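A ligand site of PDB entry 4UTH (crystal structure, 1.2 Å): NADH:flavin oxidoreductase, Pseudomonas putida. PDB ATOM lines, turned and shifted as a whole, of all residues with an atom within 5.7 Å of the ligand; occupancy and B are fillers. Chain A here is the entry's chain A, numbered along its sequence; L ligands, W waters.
An oxygen (O7) of the ligand lies within salt-bridge range of the guanidinium group (NE) of Arg 328 (2.8 Å).
The backbone NH of Arg 328 lies within hydrogen-bond range of an oxygen (O7) of the ligand, 2.8 Å away.
O2 of the ligand lies within hydrogen-bond range of SG of Cys 27 (3.3 Å).
O1 of the ligand lies within hydrogen-bond range of NE2 of His 180 (3.3 Å).
O1 of the ligand lies within hydrogen-bond range of NH1 of Arg 233, 2.8 Å away.
The backbone NH (N) of Gly 327 sits at hydrogen-bond distance from an oxygen (O9) of the ligand, 2.8 Å away.
N of Ala 59 sits at hydrogen-bond distance from O2 of the ligand.
The backbone NH (N) of Gly 305 is in hydrogen-bond range of an oxygen (O8) of the ligand (2.9 Å).
The side-chain amide oxygen of Gln 101 sits at hydrogen-bond distance from a nitrogen (N2) of the ligand (2.9 Å).
An oxygen (O3) of the ligand sits at hydrogen-bond distance from the backbone carbonyl oxygen (O) of Pro 25, 2.9 Å away.
The backbone NH (N) of Cys 27 is in hydrogen-bond range of a nitrogen (N3) of the ligand (2.9 Å).
N of Trp 304 sits at hydrogen-bond distance from O6 of the ligand (3.4 Å).
Merely in contact with the ligand: Pro 24 (3.4 Å), Met 26 (3.4 Å), Ala 303 (3.4 Å), His 183 (3.4 Å), Val 326 (3.7 Å), Glu 58 (3.9 Å) and Leu 331 (3.9 Å).
Hydrophobic or aromatic side chains within 4 Å of the ligand: Pro 24, Pro 25, Met 26, Ala 59, His 180, His 183, Ala 303, Trp 304 and Leu 331.
17 residues have an atom within 4 Å of the ligand: Pro 24, Pro 25, Met 26, Cys 27, Glu 58, Ala 59, Gln 101, His 180, His 183, Arg 233, Ala 303, Trp 304, Gly 305, Val 326, Gly 327, Arg 328 and Leu 331.
The nearest printed residue that does not touch the ligand is Ser 325 (4.2 Å).
OE1 of Glu 58 sits at hydrogen-bond distance from N of Gln 28 (2.9 Å).
The side-chain amide oxygen (OE1) of Gln 101 lies close to the backbone NH (N) of Ala 59 (3.4 Å).
O of Met 26 is in hydrogen-bond range of NE2 of Gln 28, 3.0 Å away.
A ring nitrogen (NE2) of His 183 sits at hydrogen-bond distance from the side-chain hydroxyl (OG) of Ser 268, 2.7 Å away.
The side-chain amide nitrogen (NE2) of Gln 101 lies within hydrogen-bond range of the side-chain carboxylate (OE2) of Glu 178 (2.8 Å).
Water W4 bridges an oxygen (O8) of the ligand and the guanidinium group of Arg 328.
Water W3 lies within hydrogen-bond range of O9 of the ligand (2.8 Å), N of Ala 329 (2.8 Å) and N of Arg 328 (3.4 Å).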
ATOM      1  N   PRO A  24      -6.541 -28.978   8.420  1.00  0.00           N
ATOM      2  CA  PRO A  24      -7.123 -27.658   8.571  1.00  0.00           C
ATOM      3  C   PRO A  24      -7.720 -27.507   9.958  1.00  0.00           C
ATOM      4  O   PRO A  24      -7.958 -28.513  10.644  1.00  0.00           O
ATOM      5  CB  PRO A  24      -8.199 -27.620   7.491  1.00  0.00           C
ATOM      6  CG  PRO A  24      -8.673 -29.054   7.469  1.00  0.00           C
ATOM      7  CD  PRO A  24      -7.421 -29.875   7.647  1.00  0.00           C
ATOM      8  N   PRO A  25      -8.001 -26.268  10.363  1.00  0.00           N
ATOM      9  CA  PRO A  25      -8.602 -26.051  11.665  1.00  0.00           C
ATOM     10  C   PRO A  25      -9.923 -26.773  11.784  1.00  0.00           C
ATOM     11  O   PRO A  25     -10.757 -26.695  10.897  1.00  0.00           O
ATOM     12  CB  PRO A  25      -8.802 -24.532  11.732  1.00  0.00           C
ATOM     13  CG  PRO A  25      -8.759 -24.088  10.280  1.00  0.00           C
ATOM     14  CD  PRO A  25      -7.813 -25.002   9.615  1.00  0.00           C
ATOM     15  N   MET A  26     -10.088 -27.503  12.889  1.00  0.00           N
ATOM     16  CA  MET A  26     -11.340 -28.209  13.157  1.00  0.00           C
ATOM     17  C   MET A  26     -11.729 -28.059  14.627  1.00  0.00           C
ATOM     18  O   MET A  26     -11.182 -28.745  15.500  1.00  0.00           O
ATOM     19  CB  MET A  26     -11.252 -29.698  12.796  1.00  0.00           C
ATOM     20  CG  MET A  26     -11.253 -29.948  11.282  1.00  0.00           C
ATOM     21  SD  MET A  26     -11.170 -31.706  10.886  1.00  0.00           S
ATOM     22  CE  MET A  26      -9.481 -32.061  11.327  1.00  0.00           C
ATOM     23  N   CYS A  27     -12.698 -27.193  14.867  1.00  0.00           N
ATOM     24  CA  CYS A  27     -13.293 -27.013  16.187  1.00  0.00           C
ATOM     25  C   CYS A  27     -13.650 -28.332  16.845  1.00  0.00           C
ATOM     26  O   CYS A  27     -14.232 -29.214  16.212  1.00  0.00           O
ATOM     27  CB  CYS A  27     -14.544 -26.162  16.076  1.00  0.00           C
ATOM     28  SG  CYS A  27     -14.251 -24.409  15.866  1.00  0.00           S
ATOM     29  N   GLN A  28     -13.308 -28.431  18.127  1.00  0.00           N
ATOM     30  CA  GLN A  28     -13.558 -29.610  18.931  1.00  0.00           C
ATOM     31  C   GLN A  28     -14.677 -29.405  19.951  1.00  0.00           C
ATOM     32  O   GLN A  28     -15.227 -30.369  20.470  1.00  0.00           O
ATOM     33  CB  GLN A  28     -12.264 -30.028  19.635  1.00  0.00           C
ATOM     34  CG  GLN A  28     -11.155 -30.452  18.698  1.00  0.00           C
ATOM     35  CD  GLN A  28     -11.545 -31.665  17.898  1.00  0.00           C
ATOM     36  OE1 GLN A  28     -11.599 -32.769  18.431  1.00  0.00           O
ATOM     37  NE2 GLN A  28     -11.835 -31.475  16.617  1.00  0.00           N
ATOM     38  N   TYR A  29     -14.994 -28.152  20.277  1.00  0.00           N
ATOM     39  CA  TYR A  29     -16.089 -27.805  21.169  1.00  0.00           C
ATOM     40  C   TYR A  29     -15.902 -28.392  22.574  1.00  0.00           C
ATOM     41  O   TYR A  29     -16.875 -28.690  23.255  1.00  0.00           O
ATOM     42  CB  TYR A  29     -17.450 -28.227  20.582  1.00  0.00           C
ATOM     43  CG  TYR A  29     -17.635 -27.757  19.160  1.00  0.00           C
ATOM     44  CD1 TYR A  29     -18.127 -26.485  18.882  1.00  0.00           C
ATOM     45  CD2 TYR A  29     -17.292 -28.563  18.090  1.00  0.00           C
ATOM     46  CE1 TYR A  29     -18.275 -26.049  17.564  1.00  0.00           C
ATOM     47  CE2 TYR A  29     -17.425 -28.119  16.786  1.00  0.00           C
ATOM     48  CZ  TYR A  29     -17.939 -26.877  16.533  1.00  0.00           C
ATOM     49  OH  TYR A  29     -18.069 -26.461  15.221  1.00  0.00           O
ATOM     50  N   GLU A  58      -7.742 -25.498  15.605  1.00  0.00           N
ATOM     51  CA  GLU A  58      -9.093 -24.991  15.440  1.00  0.00           C
ATOM     52  C   GLU A  58      -9.250 -23.491  15.673  1.00  0.00           C
ATOM     53  O   GLU A  58      -8.479 -22.886  16.438  1.00  0.00           O
ATOM     54  CB  GLU A  58     -10.005 -25.697  16.423  1.00  0.00           C
ATOM     55  CG  GLU A  58      -9.670 -25.455  17.896  1.00  0.00           C
ATOM     56  CD  GLU A  58     -10.346 -26.479  18.798  1.00  0.00           C
ATOM     57  OE1 GLU A  58     -11.542 -26.300  19.133  1.00  0.00           O
ATOM     58  OE2 GLU A  58      -9.688 -27.477  19.122  1.00  0.00           O
ATOM     59  N   ALA A  59     -10.312 -22.944  15.078  1.00  0.00           N
ATOM     60  CA  ALA A  59     -10.699 -21.548  15.321  1.00  0.00           C
ATOM     61  C   ALA A  59     -10.626 -21.212  16.796  1.00  0.00           C
ATOM     62  O   ALA A  59     -11.391 -21.737  17.596  1.00  0.00           O
ATOM     63  CB  ALA A  59     -12.122 -21.308  14.828  1.00  0.00           C
ATOM     64  N   GLN A 101      -5.444 -21.080  13.918  1.00  0.00           N
ATOM     65  CA  GLN A 101      -6.404 -20.185  13.288  1.00  0.00           C
ATOM     66  C   GLN A 101      -7.012 -19.290  14.352  1.00  0.00           C
ATOM     67  O   GLN A 101      -7.602 -19.803  15.312  1.00  0.00           O
ATOM     68  CB  GLN A 101      -7.491 -20.984  12.569  1.00  0.00           C
ATOM     69  CG  GLN A 101      -8.433 -20.090  11.788  1.00  0.00           C
ATOM     70  CD  GLN A 101      -9.650 -20.807  11.297  1.00  0.00           C
ATOM     71  OE1 GLN A 101     -10.409 -21.340  12.087  1.00  0.00           O
ATOM     72  NE2 GLN A 101      -9.841 -20.839   9.977  1.00  0.00           N
ATOM     73  N   GLU A 178      -3.172 -18.400  10.916  1.00  0.00           N
ATOM     74  CA  GLU A 178      -4.244 -18.223   9.947  1.00  0.00           C
ATOM     75  C   GLU A 178      -5.333 -17.320  10.499  1.00  0.00           C
ATOM     76  O   GLU A 178      -5.942 -17.619  11.535  1.00  0.00           O
ATOM     77  CB  GLU A 178      -4.827 -19.568   9.537  1.00  0.00           C
ATOM     78  CG  GLU A 178      -5.840 -19.467   8.396  1.00  0.00           C
ATOM     79  CD  GLU A 178      -6.426 -20.813   8.023  1.00  0.00           C
ATOM     80  OE1 GLU A 178      -5.708 -21.621   7.403  1.00  0.00           O
ATOM     81  OE2 GLU A 178      -7.603 -21.073   8.318  1.00  0.00           O
ATOM     82  N   HIS A 180      -8.959 -16.077  10.450  1.00  0.00           N
ATOM     83  CA  HIS A 180     -10.218 -16.648   9.999  1.00  0.00           C
ATOM     84  C   HIS A 180     -11.149 -15.597   9.437  1.00  0.00           C
ATOM     85  O   HIS A 180     -11.996 -15.046  10.157  1.00  0.00           O
ATOM     86  CB  HIS A 180     -10.918 -17.393  11.122  1.00  0.00           C
ATOM     87  CG  HIS A 180     -11.965 -18.337  10.631  1.00  0.00           C
ATOM     88  ND1 HIS A 180     -12.403 -18.355   9.318  1.00  0.00           N
ATOM     89  CD2 HIS A 180     -12.613 -19.338  11.267  1.00  0.00           C
ATOM     90  CE1 HIS A 180     -13.272 -19.322   9.177  1.00  0.00           C
ATOM     91  NE2 HIS A 180     -13.422 -19.948  10.337  1.00  0.00           N
ATOM     92  N   HIS A 183     -16.311 -18.198   6.186  1.00  0.00           N
ATOM     93  CA  HIS A 183     -17.387 -18.987   6.803  1.00  0.00           C
ATOM     94  C   HIS A 183     -18.410 -18.123   7.548  1.00  0.00           C
ATOM     95  O   HIS A 183     -19.084 -18.570   8.488  1.00  0.00           O
ATOM     96  CB  HIS A 183     -16.785 -20.071   7.707  1.00  0.00           C
ATOM     97  CG  HIS A 183     -15.880 -21.002   6.970  1.00  0.00           C
ATOM     98  ND1 HIS A 183     -15.123 -21.961   7.601  1.00  0.00           N
ATOM     99  CD2 HIS A 183     -15.623 -21.142   5.650  1.00  0.00           C
ATOM    100  CE1 HIS A 183     -14.418 -22.634   6.700  1.00  0.00           C
ATOM    101  NE2 HIS A 183     -14.721 -22.168   5.504  1.00  0.00           N
ATOM    102  N   ARG A 233      -7.834 -17.533   5.928  1.00  0.00           N
ATOM    103  CA  ARG A 233      -8.881 -18.294   5.256  1.00  0.00           C
ATOM    104  C   ARG A 233      -9.924 -17.270   4.824  1.00  0.00           C
ATOM    105  O   ARG A 233     -10.288 -16.390   5.591  1.00  0.00           O
ATOM    106  CB  ARG A 233      -9.473 -19.362   6.155  1.00  0.00           C
ATOM    107  CG  ARG A 233     -10.250 -20.441   5.367  1.00  0.00           C
ATOM    108  CD  ARG A 233     -10.573 -21.669   6.177  1.00  0.00           C
ATOM    109  NE  ARG A 233     -10.613 -22.853   5.320  1.00  0.00           N
ATOM    110  CZ  ARG A 233     -10.879 -24.082   5.735  1.00  0.00           C
ATOM    111  NH1 ARG A 233     -11.230 -24.301   6.995  1.00  0.00           N
ATOM    112  NH2 ARG A 233     -10.818 -25.090   4.872  1.00  0.00           N
ATOM    113  N   SER A 268     -11.886 -20.808   0.551  1.00  0.00           N
ATOM    114  CA  SER A 268     -13.076 -21.492   0.978  1.00  0.00           C
ATOM    115  C   SER A 268     -14.326 -20.839   0.375  1.00  0.00           C
ATOM    116  O   SER A 268     -14.244 -20.005  -0.554  1.00  0.00           O
ATOM    117  CB  SER A 268     -13.135 -21.522   2.508  1.00  0.00           C
ATOM    118  OG  SER A 268     -14.053 -22.503   2.950  1.00  0.00           O
ATOM    119  N   ALA A 303     -10.058 -27.238   0.764  1.00  0.00           N
ATOM    120  CA  ALA A 303     -10.542 -28.409   1.453  1.00  0.00           C
ATOM    121  C   ALA A 303     -11.887 -28.807   0.870  1.00  0.00           C
ATOM    122  O   ALA A 303     -12.458 -28.072   0.074  1.00  0.00           O
ATOM    123  CB  ALA A 303     -10.654 -28.133   2.957  1.00  0.00           C
ATOM    124  N   TRP A 304     -12.334 -29.975   1.302  1.00  0.00           N
ATOM    125  CA  TRP A 304     -13.642 -30.599   1.104  1.00  0.00           C
ATOM    126  C   TRP A 304     -13.479 -31.764   0.152  1.00  0.00           C
ATOM    127  O   TRP A 304     -13.453 -31.620  -1.082  1.00  0.00           O
ATOM    128  CB  TRP A 304     -14.731 -29.669   0.610  1.00  0.00           C
ATOM    129  CG  TRP A 304     -16.045 -30.414   0.692  1.00  0.00           C
ATOM    130  CD1 TRP A 304     -16.562 -31.345  -0.203  1.00  0.00           C
ATOM    131  CD2 TRP A 304     -16.974 -30.347   1.761  1.00  0.00           C
ATOM    132  NE1 TRP A 304     -17.762 -31.823   0.252  1.00  0.00           N
ATOM    133  CE2 TRP A 304     -18.029 -31.234   1.458  1.00  0.00           C
ATOM    134  CE3 TRP A 304     -17.032 -29.609   2.951  1.00  0.00           C
ATOM    135  CZ2 TRP A 304     -19.131 -31.393   2.309  1.00  0.00           C
ATOM    136  CZ3 TRP A 304     -18.117 -29.769   3.785  1.00  0.00           C
ATOM    137  CH2 TRP A 304     -19.159 -30.661   3.455  1.00  0.00           C
ATOM    138  N   GLY A 305     -13.365 -32.937   0.749  1.00  0.00           N
ATOM    139  CA  GLY A 305     -13.309 -34.171  -0.004  1.00  0.00           C
ATOM    140  C   GLY A 305     -11.957 -34.571  -0.544  1.00  0.00           C
ATOM    141  O   GLY A 305     -11.898 -35.413  -1.443  1.00  0.00           O
ATOM    142  N   PHE A 306     -10.862 -34.018  -0.011  1.00  0.00           N
ATOM    143  CA  PHE A 306      -9.546 -34.380  -0.513  1.00  0.00           C
ATOM    144  C   PHE A 306      -8.948 -35.573   0.251  1.00  0.00           C
ATOM    145  O   PHE A 306      -7.811 -35.956  -0.005  1.00  0.00           O
ATOM    146  CB  PHE A 306      -8.573 -33.198  -0.449  1.00  0.00           C
ATOM    147  CG  PHE A 306      -8.817 -32.126  -1.475  1.00  0.00           C
ATOM    148  CD1 PHE A 306      -8.352 -32.254  -2.767  1.00  0.00           C
ATOM    149  CD2 PHE A 306      -9.494 -30.950  -1.133  1.00  0.00           C
ATOM    150  CE1 PHE A 306      -8.550 -31.251  -3.709  1.00  0.00           C
ATOM    151  CE2 PHE A 306      -9.705 -29.950  -2.080  1.00  0.00           C
ATOM    152  CZ  PHE A 306      -9.231 -30.098  -3.364  1.00  0.00           C
ATOM    153  N   GLY A 307      -9.714 -36.169   1.165  1.00  0.00           N
ATOM    154  CA  GLY A 307      -9.296 -37.385   1.849  1.00  0.00           C
ATOM    155  C   GLY A 307      -9.141 -38.648   1.005  1.00  0.00           C
ATOM    156  O   GLY A 307      -8.791 -39.699   1.507  1.00  0.00           O
ATOM    157  N   SER A 325      -5.606 -29.649   2.183  1.00  0.00           N
ATOM    158  CA  SER A 325      -6.188 -29.708   3.518  1.00  0.00           C
ATOM    159  C   SER A 325      -7.140 -30.897   3.597  1.00  0.00           C
ATOM    160  O   SER A 325      -8.043 -31.022   2.793  1.00  0.00           O
ATOM    161  CB  SER A 325      -6.906 -28.421   3.846  1.00  0.00           C
ATOM    162  OG  SER A 325      -5.963 -27.366   3.909  1.00  0.00           O
ATOM    163  N   VAL A 326      -6.912 -31.735   4.600  1.00  0.00           N
ATOM    164  CA  VAL A 326      -7.648 -32.974   4.801  1.00  0.00           C
ATOM    165  C   VAL A 326      -8.177 -32.988   6.235  1.00  0.00           C
ATOM    166  O   VAL A 326      -7.394 -33.160   7.172  1.00  0.00           O
ATOM    167  CB  VAL A 326      -6.753 -34.190   4.538  1.00  0.00           C
ATOM    168  CG1 VAL A 326      -7.520 -35.485   4.795  1.00  0.00           C
ATOM    169  CG2 VAL A 326      -6.210 -34.177   3.123  1.00  0.00           C
ATOM    170  N   GLY A 327      -9.472 -32.785   6.386  1.00  0.00           N
ATOM    171  CA  GLY A 327     -10.091 -32.610   7.694  1.00  0.00           C
ATOM    172  C   GLY A 327     -10.740 -33.863   8.248  1.00  0.00           C
ATOM    173  O   GLY A 327     -10.153 -34.566   9.080  1.00  0.00           O
ATOM    174  N   ARG A 328     -11.965 -34.164   7.819  1.00  0.00           N
ATOM    175  CA  ARG A 328     -12.717 -35.272   8.422  1.00  0.00           C
ATOM    176  C   ARG A 328     -12.025 -36.626   8.325  1.00  0.00           C
ATOM    177  O   ARG A 328     -12.166 -37.443   9.254  1.00  0.00           O
ATOM    178  CB  ARG A 328     -14.115 -35.335   7.783  1.00  0.00           C
ATOM    179  CG  ARG A 328     -15.045 -34.264   8.362  1.00  0.00           C
ATOM    180  CD  ARG A 328     -16.314 -34.103   7.606  1.00  0.00           C
ATOM    181  NE  ARG A 328     -16.032 -33.566   6.281  1.00  0.00           N
ATOM    182  CZ  ARG A 328     -16.972 -33.336   5.379  1.00  0.00           C
ATOM    183  NH1 ARG A 328     -18.237 -33.598   5.658  1.00  0.00           N
ATOM    184  NH2 ARG A 328     -16.631 -32.869   4.195  1.00  0.00           N
ATOM    185  N   ALA A 329     -11.248 -36.863   7.264  1.00  0.00           N
ATOM    186  CA  ALA A 329     -10.546 -38.132   7.173  1.00  0.00           C
ATOM    187  C   ALA A 329      -9.568 -38.321   8.341  1.00  0.00           C
ATOM    188  O   ALA A 329      -9.278 -39.443   8.737  1.00  0.00           O
ATOM    189  CB  ALA A 329      -9.808 -38.241   5.857  1.00  0.00           C
ATOM    190  N   LEU A 331     -10.203 -37.109  11.424  1.00  0.00           N
ATOM    191  CA  LEU A 331     -11.030 -37.463  12.571  1.00  0.00           C
ATOM    192  C   LEU A 331     -11.304 -38.971  12.533  1.00  0.00           C
ATOM    193  O   LEU A 331     -11.264 -39.640  13.554  1.00  0.00           O
ATOM    194  CB  LEU A 331     -12.336 -36.683  12.569  1.00  0.00           C
ATOM    195  CG  LEU A 331     -12.208 -35.165  12.508  1.00  0.00           C
ATOM    196  CD1 LEU A 331     -13.573 -34.505  12.549  1.00  0.00           C
ATOM    197  CD2 LEU A 331     -11.311 -34.598  13.589  1.00  0.00           C
HETATM  198  N1  LIG L   1     -13.017 -24.570   9.333  1.00  0.00           N
HETATM  199  C1  LIG L   1     -12.334 -23.528   9.837  1.00  0.00           C
HETATM  200  O1  LIG L   1     -11.946 -22.587   9.086  1.00  0.00           O
HETATM  201  N2  LIG L   1     -12.250 -23.365  11.203  1.00  0.00           N
HETATM  202  C2  LIG L   1     -12.523 -24.344  12.080  1.00  0.00           C
HETATM  203  O2  LIG L   1     -12.277 -24.259  13.265  1.00  0.00           O
HETATM  204  C3  LIG L   1     -13.458 -25.364  11.557  1.00  0.00           C
HETATM  205  N3  LIG L   1     -14.011 -26.262  12.414  1.00  0.00           N
HETATM  206  C4  LIG L   1     -14.415 -27.469  11.871  1.00  0.00           C
HETATM  207  C5  LIG L   1     -14.746 -28.523  12.752  1.00  0.00           C
HETATM  208  C6  LIG L   1     -15.007 -29.795  12.257  1.00  0.00           C
HETATM  209  C7  LIG L   1     -15.093 -30.926  13.180  1.00  0.00           C
HETATM  210  C8  LIG L   1     -15.048 -29.995  10.836  1.00  0.00           C
HETATM  211  C9  LIG L   1     -15.367 -31.355  10.267  1.00  0.00           C
HETATM  212  C10 LIG L   1     -14.937 -28.892  10.005  1.00  0.00           C
HETATM  213  C11 LIG L   1     -14.465 -27.662  10.498  1.00  0.00           C
HETATM  214  N4  LIG L   1     -14.086 -26.639   9.630  1.00  0.00           N
HETATM  215  C12 LIG L   1     -13.547 -25.504  10.191  1.00  0.00           C
HETATM  216  C13 LIG L   1     -13.915 -26.882   8.170  1.00  0.00           C
HETATM  217  C14 LIG L   1     -12.691 -27.752   7.902  1.00  0.00           C
HETATM  218  O3  LIG L   1     -11.478 -27.044   8.109  1.00  0.00           O
HETATM  219  C15 LIG L   1     -12.686 -28.272   6.446  1.00  0.00           C
HETATM  220  O4  LIG L   1     -12.662 -27.158   5.543  1.00  0.00           O
HETATM  221  C16 LIG L   1     -13.887 -29.144   6.089  1.00  0.00           C
HETATM  222  O5  LIG L   1     -14.051 -30.196   7.055  1.00  0.00           O
HETATM  223  C17 LIG L   1     -13.745 -29.777   4.699  1.00  0.00           C
HETATM  224  O6  LIG L   1     -12.629 -30.665   4.577  1.00  0.00           O
HETATM  225  P1  LIG L   1     -12.847 -32.273   4.650  1.00  0.00           P
HETATM  226  O7  LIG L   1     -13.401 -32.547   6.041  1.00  0.00           O
HETATM  227  O8  LIG L   1     -13.816 -32.647   3.567  1.00  0.00           O
HETATM  228  O9  LIG L   1     -11.451 -32.788   4.465  1.00  0.00           O
HETATM  229  O   HOH W   1     -17.468 -27.806   8.322  1.00  0.00           O
HETATM  230  O   HOH W   2     -10.530 -31.996   2.094  1.00  0.00           O
HETATM  231  O   HOH W   3     -11.193 -35.538   4.758  1.00  0.00           O
HETATM  232  O   HOH W   4     -14.535 -35.282   3.281  1.00  0.00           O
